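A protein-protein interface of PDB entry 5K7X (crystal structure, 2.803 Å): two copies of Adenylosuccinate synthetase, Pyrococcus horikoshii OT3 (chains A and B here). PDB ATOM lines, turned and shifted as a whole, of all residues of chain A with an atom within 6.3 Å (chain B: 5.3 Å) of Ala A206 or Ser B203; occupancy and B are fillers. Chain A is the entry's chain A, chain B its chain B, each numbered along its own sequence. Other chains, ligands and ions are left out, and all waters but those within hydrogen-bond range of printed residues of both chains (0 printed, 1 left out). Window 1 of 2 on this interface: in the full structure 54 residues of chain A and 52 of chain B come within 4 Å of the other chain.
Tyr A187 touches Asp B207, and with the chains exchanged Asp A207 touches Tyr B187.
Ser A202 touches its own counterpart, Ser B202.
Ser A202 touches Ala B205, and with the chains exchanged Ala A205 touches Ser B202.
Ser A203 touches Ala B206, and with the chains exchanged Ala A206 touches Ser B203.
Of the 19 pairs that touch across the chains among the printed residues, 11 have their exchanged pair printed and touching as well.
CA of Gly A74 touches CE2 of Tyr B187 (3.6 Å).
CD2 of Tyr A187 touches O of Ala B206 (3.9 Å).
Ser B202 touches Ser A202 (O to CB, 3.3 Å).
Ser A202 touches Ala B206.
CB of Ala B206 touches OG of Ser A203 (3.4 Å).
Ala A205 touches Ser B202.
Ala A206 touches Tyr B187 (O to CD2, 3.9 Å).
Ala A206 touches Asp B198 (CB to OD2, 3.3 Å).
Asp A207 touches Tyr B187 (OD1 to CE2, 3.6 Å).
Val A208 touches Tyr B188 (C to OH, 3.3 Å).
The backbone NH of Gly A74 sits at hydrogen-bond distance from the backbone carbonyl oxygen of Asp A207.
N of Ala A73 is in hydrogen-bond range of O of Asp A207, 3.0 Å away.
The side-chain carboxylate of Asp B198 sits at hydrogen-bond distance from the side-chain hydroxyl of Thr B200, at 2.7 Å.
The backbone carbonyl oxygen (O) of Ala A205 lies within hydrogen-bond range of the backbone NH (N) of Ile A210 (2.8 Å).
The backbone NH of Gly A209 lies within hydrogen-bond range of the side-chain hydroxyl of Tyr B188 (2.9 Å).
O of Ile A210 lies within hydrogen-bond range of OG of Ser B202, 2.6 Å away.
The backbone carbonyl oxygen of Asp A207 is in hydrogen-bond range of the side-chain hydroxyl of Tyr B188, 3.1 Å away.
O of Ala A206 is in hydrogen-bond range of OH of Tyr B188 (2.6 Å).
Printed residues of chain A that touch a printed residue of chain B: Ala A73, Gly A74, Tyr A187, Ser A202, Ser A203, Ala A205, Ala A206, Asp A207, Val A208, Gly A209 and Ile A210.
Of the 12 printed residues of chain B, 8 touch a printed residue of chain A.
Among the printed residues, 19 pairs touch across the chains.
Among the printed residues, no Asp or Glu carboxylate lies within 4 Å of a Lys or Arg side-chain nitrogen of the other chain.
Ala A206 touches just these residues of chain B: Tyr B187 (3.9 Å), Tyr B188 (2.6 Å), Asp B198 (3.3 Å), Ser B202 (3.6 Å) and Ser B203 (3.4 Å).
Ser B203 touches just one residue of chain A: Ala A206 (3.4 Å).
Of the printed residues of chain B, Ser A202 touches Ser B202 (3.3 Å), Ala B205 (3.6 Å) and Ala B206 (3.6 Å).
Printed residues of chain A within 4 Å of Asp B207: Tyr A187.
Printed residues of chain B within 4 Å of Val A208: Tyr B188.
Printed residues of chain B within 4 Å of Ala A205: Ser B202.
Thr B200 touches none of the printed residues of chain A.
The nearest residue of chain B that does not touch Ala A206 is Thr B200 (4.1 Å).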
ATOM      1  N   ALA A  73     -32.998 -30.355   8.547  1.00  0.00           N
ATOM      2  CA  ALA A  73     -33.750 -29.166   8.939  1.00  0.00           C
ATOM      3  C   ALA A  73     -32.888 -27.907   9.018  1.00  0.00           C
ATOM      4  O   ALA A  73     -33.382 -26.798   8.818  1.00  0.00           O
ATOM      5  CB  ALA A  73     -34.439 -29.408  10.272  1.00  0.00           C
ATOM      6  N   GLY A  74     -31.604 -28.081   9.309  1.00  0.00           N
ATOM      7  CA  GLY A  74     -30.693 -26.956   9.430  1.00  0.00           C
ATOM      8  C   GLY A  74     -30.278 -26.362   8.096  1.00  0.00           C
ATOM      9  O   GLY A  74     -29.587 -25.346   8.043  1.00  0.00           O
ATOM     10  N   TYR A 187     -17.700 -19.618  12.658  1.00  0.00           N
ATOM     11  CA  TYR A 187     -17.029 -19.529  13.953  1.00  0.00           C
ATOM     12  C   TYR A 187     -15.513 -19.546  13.802  1.00  0.00           C
ATOM     13  O   TYR A 187     -14.822 -18.645  14.278  1.00  0.00           O
ATOM     14  CB  TYR A 187     -17.452 -20.677  14.877  1.00  0.00           C
ATOM     15  CG  TYR A 187     -18.933 -20.759  15.172  1.00  0.00           C
ATOM     16  CD1 TYR A 187     -19.771 -19.671  14.960  1.00  0.00           C
ATOM     17  CD2 TYR A 187     -19.493 -21.933  15.656  1.00  0.00           C
ATOM     18  CE1 TYR A 187     -21.123 -19.753  15.224  1.00  0.00           C
ATOM     19  CE2 TYR A 187     -20.843 -22.024  15.921  1.00  0.00           C
ATOM     20  CZ  TYR A 187     -21.654 -20.934  15.704  1.00  0.00           C
ATOM     21  OH  TYR A 187     -23.002 -21.024  15.969  1.00  0.00           O
ATOM     22  N   ALA A 201     -18.031 -30.729  11.442  1.00  0.00           N
ATOM     23  CA  ALA A 201     -18.782 -31.980  11.522  1.00  0.00           C
ATOM     24  C   ALA A 201     -19.875 -31.957  12.586  1.00  0.00           C
ATOM     25  O   ALA A 201     -20.926 -32.574  12.418  1.00  0.00           O
ATOM     26  CB  ALA A 201     -17.831 -33.144  11.779  1.00  0.00           C
ATOM     27  N   SER A 202     -19.623 -31.260  13.688  1.00  0.00           N
ATOM     28  CA  SER A 202     -20.610 -31.169  14.753  1.00  0.00           C
ATOM     29  C   SER A 202     -21.845 -30.405  14.286  1.00  0.00           C
ATOM     30  O   SER A 202     -22.976 -30.807  14.564  1.00  0.00           O
ATOM     31  CB  SER A 202     -20.006 -30.502  15.989  1.00  0.00           C
ATOM     32  OG  SER A 202     -19.119 -31.383  16.655  1.00  0.00           O
ATOM     33  N   SER A 203     -21.623 -29.316  13.557  1.00  0.00           N
ATOM     34  CA  SER A 203     -22.723 -28.527  13.012  1.00  0.00           C
ATOM     35  C   SER A 203     -23.525 -29.326  11.992  1.00  0.00           C
ATOM     36  O   SER A 203     -24.756 -29.300  12.002  1.00  0.00           O
ATOM     37  CB  SER A 203     -22.198 -27.242  12.368  1.00  0.00           C
ATOM     38  OG  SER A 203     -21.733 -26.338  13.350  1.00  0.00           O
ATOM     39  N   VAL A 204     -22.820 -30.041  11.120  1.00  0.00           N
ATOM     40  CA  VAL A 204     -23.460 -30.864  10.102  1.00  0.00           C
ATOM     41  C   VAL A 204     -24.343 -31.939  10.735  1.00  0.00           C
ATOM     42  O   VAL A 204     -25.432 -32.234  10.239  1.00  0.00           O
ATOM     43  CB  VAL A 204     -22.412 -31.525   9.185  1.00  0.00           C
ATOM     44  CG1 VAL A 204     -23.085 -32.396   8.143  1.00  0.00           C
ATOM     45  CG2 VAL A 204     -21.562 -30.461   8.510  1.00  0.00           C
ATOM     46  N   ALA A 205     -23.877 -32.509  11.841  1.00  0.00           N
ATOM     47  CA  ALA A 205     -24.656 -33.502  12.573  1.00  0.00           C
ATOM     48  C   ALA A 205     -25.940 -32.878  13.109  1.00  0.00           C
ATOM     49  O   ALA A 205     -27.005 -33.493  13.068  1.00  0.00           O
ATOM     50  CB  ALA A 205     -23.838 -34.094  13.706  1.00  0.00           C
ATOM     51  N   ALA A 206     -25.834 -31.649  13.605  1.00  0.00           N
ATOM     52  CA  ALA A 206     -26.996 -30.945  14.129  1.00  0.00           C
ATOM     53  C   ALA A 206     -27.961 -30.573  13.007  1.00  0.00           C
ATOM     54  O   ALA A 206     -29.164 -30.447  13.227  1.00  0.00           O
ATOM     55  CB  ALA A 206     -26.565 -29.700  14.892  1.00  0.00           C
ATOM     56  N   ASP A 207     -27.427 -30.411  11.801  1.00  0.00           N
ATOM     57  CA  ASP A 207     -28.235 -30.010  10.655  1.00  0.00           C
ATOM     58  C   ASP A 207     -29.226 -31.093  10.259  1.00  0.00           C
ATOM     59  O   ASP A 207     -30.362 -30.803   9.882  1.00  0.00           O
ATOM     60  CB  ASP A 207     -27.340 -29.674   9.460  1.00  0.00           C
ATOM     61  CG  ASP A 207     -26.524 -28.425   9.682  1.00  0.00           C
ATOM     62  OD1 ASP A 207     -26.922 -27.608  10.540  1.00  0.00           O
ATOM     63  OD2 ASP A 207     -25.486 -28.263   9.003  1.00  0.00           O
ATOM     64  N   VAL A 208     -28.786 -32.343  10.340  1.00  0.00           N
ATOM     65  CA  VAL A 208     -29.610 -33.468   9.928  1.00  0.00           C
ATOM     66  C   VAL A 208     -30.395 -34.057  11.102  1.00  0.00           C
ATOM     67  O   VAL A 208     -31.405 -34.735  10.905  1.00  0.00           O
ATOM     68  CB  VAL A 208     -28.755 -34.563   9.271  1.00  0.00           C
ATOM     69  CG1 VAL A 208     -28.304 -34.110   7.893  1.00  0.00           C
ATOM     70  CG2 VAL A 208     -27.553 -34.892  10.137  1.00  0.00           C
ATOM     71  N   GLY A 209     -29.927 -33.799  12.320  1.00  0.00           N
ATOM     72  CA  GLY A 209     -30.619 -34.255  13.514  1.00  0.00           C
ATOM     73  C   GLY A 209     -29.988 -35.467  14.175  1.00  0.00           C
ATOM     74  O   GLY A 209     -30.680 -36.410  14.554  1.00  0.00           O
ATOM     75  N   ILE A 210     -28.671 -35.427  14.335  1.00  0.00           N
ATOM     76  CA  ILE A 210     -27.924 -36.537  14.908  1.00  0.00           C
ATOM     77  C   ILE A 210     -27.087 -36.079  16.095  1.00  0.00           C
ATOM     78  O   ILE A 210     -26.286 -35.152  15.973  1.00  0.00           O
ATOM     79  CB  ILE A 210     -26.991 -37.176  13.872  1.00  0.00           C
ATOM     80  CG1 ILE A 210     -27.381 -36.759  12.459  1.00  0.00           C
ATOM     81  CG2 ILE A 210     -27.019 -38.681  13.982  1.00  0.00           C
ATOM     82  CD1 ILE A 210     -26.439 -37.308  11.407  1.00  0.00           C
ATOM     83  N   TYR B 187     -33.877 -24.947  14.942  1.00  0.00           N
ATOM     84  CA  TYR B 187     -34.216 -25.944  13.937  1.00  0.00           C
ATOM     85  C   TYR B 187     -35.415 -26.786  14.361  1.00  0.00           C
ATOM     86  O   TYR B 187     -36.420 -26.859  13.654  1.00  0.00           O
ATOM     87  CB  TYR B 187     -33.022 -26.866  13.660  1.00  0.00           C
ATOM     88  CG  TYR B 187     -31.772 -26.175  13.154  1.00  0.00           C
ATOM     89  CD1 TYR B 187     -31.824 -24.897  12.610  1.00  0.00           C
ATOM     90  CD2 TYR B 187     -30.536 -26.812  13.212  1.00  0.00           C
ATOM     91  CE1 TYR B 187     -30.679 -24.271  12.146  1.00  0.00           C
ATOM     92  CE2 TYR B 187     -29.390 -26.195  12.749  1.00  0.00           C
ATOM     93  CZ  TYR B 187     -29.465 -24.926  12.218  1.00  0.00           C
ATOM     94  OH  TYR B 187     -28.324 -24.309  11.760  1.00  0.00           O
ATOM     95  N   TYR B 188     -35.301 -27.418  15.526  1.00  0.00           N
ATOM     96  CA  TYR B 188     -36.235 -28.462  15.930  1.00  0.00           C
ATOM     97  C   TYR B 188     -37.231 -28.022  17.003  1.00  0.00           C
ATOM     98  O   TYR B 188     -38.121 -28.784  17.386  1.00  0.00           O
ATOM     99  CB  TYR B 188     -35.451 -29.682  16.414  1.00  0.00           C
ATOM    100  CG  TYR B 188     -34.398 -30.133  15.430  1.00  0.00           C
ATOM    101  CD1 TYR B 188     -34.744 -30.874  14.310  1.00  0.00           C
ATOM    102  CD2 TYR B 188     -33.061 -29.806  15.611  1.00  0.00           C
ATOM    103  CE1 TYR B 188     -33.791 -31.284  13.401  1.00  0.00           C
ATOM    104  CE2 TYR B 188     -32.099 -30.209  14.707  1.00  0.00           C
ATOM    105  CZ  TYR B 188     -32.469 -30.950  13.602  1.00  0.00           C
ATOM    106  OH  TYR B 188     -31.519 -31.360  12.692  1.00  0.00           O
ATOM    107  N   ASP B 198     -29.590 -23.308  17.023  1.00  0.00           N
ATOM    108  CA  ASP B 198     -29.824 -24.676  17.471  1.00  0.00           C
ATOM    109  C   ASP B 198     -29.107 -24.888  18.798  1.00  0.00           C
ATOM    110  O   ASP B 198     -28.053 -24.303  19.045  1.00  0.00           O
ATOM    111  CB  ASP B 198     -29.354 -25.700  16.437  1.00  0.00           C
ATOM    112  CG  ASP B 198     -29.616 -27.136  16.877  1.00  0.00           C
ATOM    113  OD1 ASP B 198     -30.749 -27.441  17.306  1.00  0.00           O
ATOM    114  OD2 ASP B 198     -28.681 -27.958  16.813  1.00  0.00           O
ATOM    115  N   VAL B 199     -29.677 -25.737  19.643  1.00  0.00           N
ATOM    116  CA  VAL B 199     -29.252 -25.822  21.031  1.00  0.00           C
ATOM    117  C   VAL B 199     -28.881 -27.263  21.420  1.00  0.00           C
ATOM    118  O   VAL B 199     -28.271 -27.504  22.467  1.00  0.00           O
ATOM    119  CB  VAL B 199     -30.373 -25.226  21.939  1.00  0.00           C
ATOM    120  CG1 VAL B 199     -30.724 -26.116  23.133  1.00  0.00           C
ATOM    121  CG2 VAL B 199     -30.004 -23.811  22.369  1.00  0.00           C
ATOM    122  N   THR B 200     -29.193 -28.211  20.538  1.00  0.00           N
ATOM    123  CA  THR B 200     -28.849 -29.617  20.756  1.00  0.00           C
ATOM    124  C   THR B 200     -27.356 -29.824  20.990  1.00  0.00           C
ATOM    125  O   THR B 200     -26.540 -28.950  20.694  1.00  0.00           O
ATOM    126  CB  THR B 200     -29.273 -30.500  19.573  1.00  0.00           C
ATOM    127  OG1 THR B 200     -28.536 -30.124  18.405  1.00  0.00           O
ATOM    128  CG2 THR B 200     -30.765 -30.359  19.307  1.00  0.00           C
ATOM    129  N   ALA B 201     -27.010 -31.004  21.495  1.00  0.00           N
ATOM    130  CA  ALA B 201     -25.642 -31.311  21.898  1.00  0.00           C
ATOM    131  C   ALA B 201     -24.631 -31.151  20.763  1.00  0.00           C
ATOM    132  O   ALA B 201     -23.489 -30.758  20.997  1.00  0.00           O
ATOM    133  CB  ALA B 201     -25.574 -32.722  22.461  1.00  0.00           C
ATOM    134  N   SER B 202     -25.047 -31.454  19.539  1.00  0.00           N
ATOM    135  CA  SER B 202     -24.159 -31.332  18.388  1.00  0.00           C
ATOM    136  C   SER B 202     -23.777 -29.875  18.152  1.00  0.00           C
ATOM    137  O   SER B 202     -22.621 -29.565  17.856  1.00  0.00           O
ATOM    138  CB  SER B 202     -24.812 -31.921  17.138  1.00  0.00           C
ATOM    139  OG  SER B 202     -24.821 -33.335  17.194  1.00  0.00           O
ATOM    140  N   SER B 203     -24.756 -28.987  18.285  1.00  0.00           N
ATOM    141  CA  SER B 203     -24.505 -27.559  18.155  1.00  0.00           C
ATOM    142  C   SER B 203     -23.605 -27.078  19.286  1.00  0.00           C
ATOM    143  O   SER B 203     -22.665 -26.313  19.062  1.00  0.00           O
ATOM    144  CB  SER B 203     -25.818 -26.779  18.144  1.00  0.00           C
ATOM    145  OG  SER B 203     -26.514 -27.000  16.931  1.00  0.00           O
ATOM    146  N   VAL B 204     -23.893 -27.541  20.499  1.00  0.00           N
ATOM    147  CA  VAL B 204     -23.095 -27.195  21.669  1.00  0.00           C
ATOM    148  C   VAL B 204     -21.649 -27.657  21.491  1.00  0.00           C
ATOM    149  O   VAL B 204     -20.709 -26.954  21.865  1.00  0.00           O
ATOM    150  CB  VAL B 204     -23.684 -27.817  22.949  1.00  0.00           C
ATOM    151  CG1 VAL B 204     -22.832 -27.465  24.155  1.00  0.00           C
ATOM    152  CG2 VAL B 204     -25.107 -27.339  23.155  1.00  0.00           C
ATOM    153  N   ALA B 205     -21.480 -28.834  20.897  1.00  0.00           N
ATOM    154  CA  ALA B 205     -20.151 -29.361  20.604  1.00  0.00           C
ATOM    155  C   ALA B 205     -19.417 -28.466  19.611  1.00  0.00           C
ATOM    156  O   ALA B 205     -18.220 -28.223  19.748  1.00  0.00           O
ATOM    157  CB  ALA B 205     -20.246 -30.781  20.067  1.00  0.00           C
ATOM    158  N   ALA B 206     -20.143 -27.978  18.610  1.00  0.00           N
ATOM    159  CA  ALA B 206     -19.556 -27.096  17.608  1.00  0.00           C
ATOM    160  C   ALA B 206     -19.209 -25.739  18.206  1.00  0.00           C
ATOM    161  O   ALA B 206     -18.293 -25.066  17.740  1.00  0.00           O
ATOM    162  CB  ALA B 206     -20.502 -26.923  16.430  1.00  0.00           C
ATOM    163  N   ASP B 207     -19.932 -25.350  19.251  1.00  0.00           N
ATOM    164  CA  ASP B 207     -19.732 -24.045  19.873  1.00  0.00           C
ATOM    165  C   ASP B 207     -18.375 -23.942  20.550  1.00  0.00           C
ATOM    166  O   ASP B 207     -17.737 -22.891  20.513  1.00  0.00           O
ATOM    167  CB  ASP B 207     -20.837 -23.754  20.891  1.00  0.00           C
ATOM    168  CG  ASP B 207     -22.185 -23.546  20.239  1.00  0.00           C
ATOM    169  OD1 ASP B 207     -22.213 -23.238  19.029  1.00  0.00           O
ATOM    170  OD2 ASP B 207     -23.213 -23.677  20.939  1.00  0.00           O
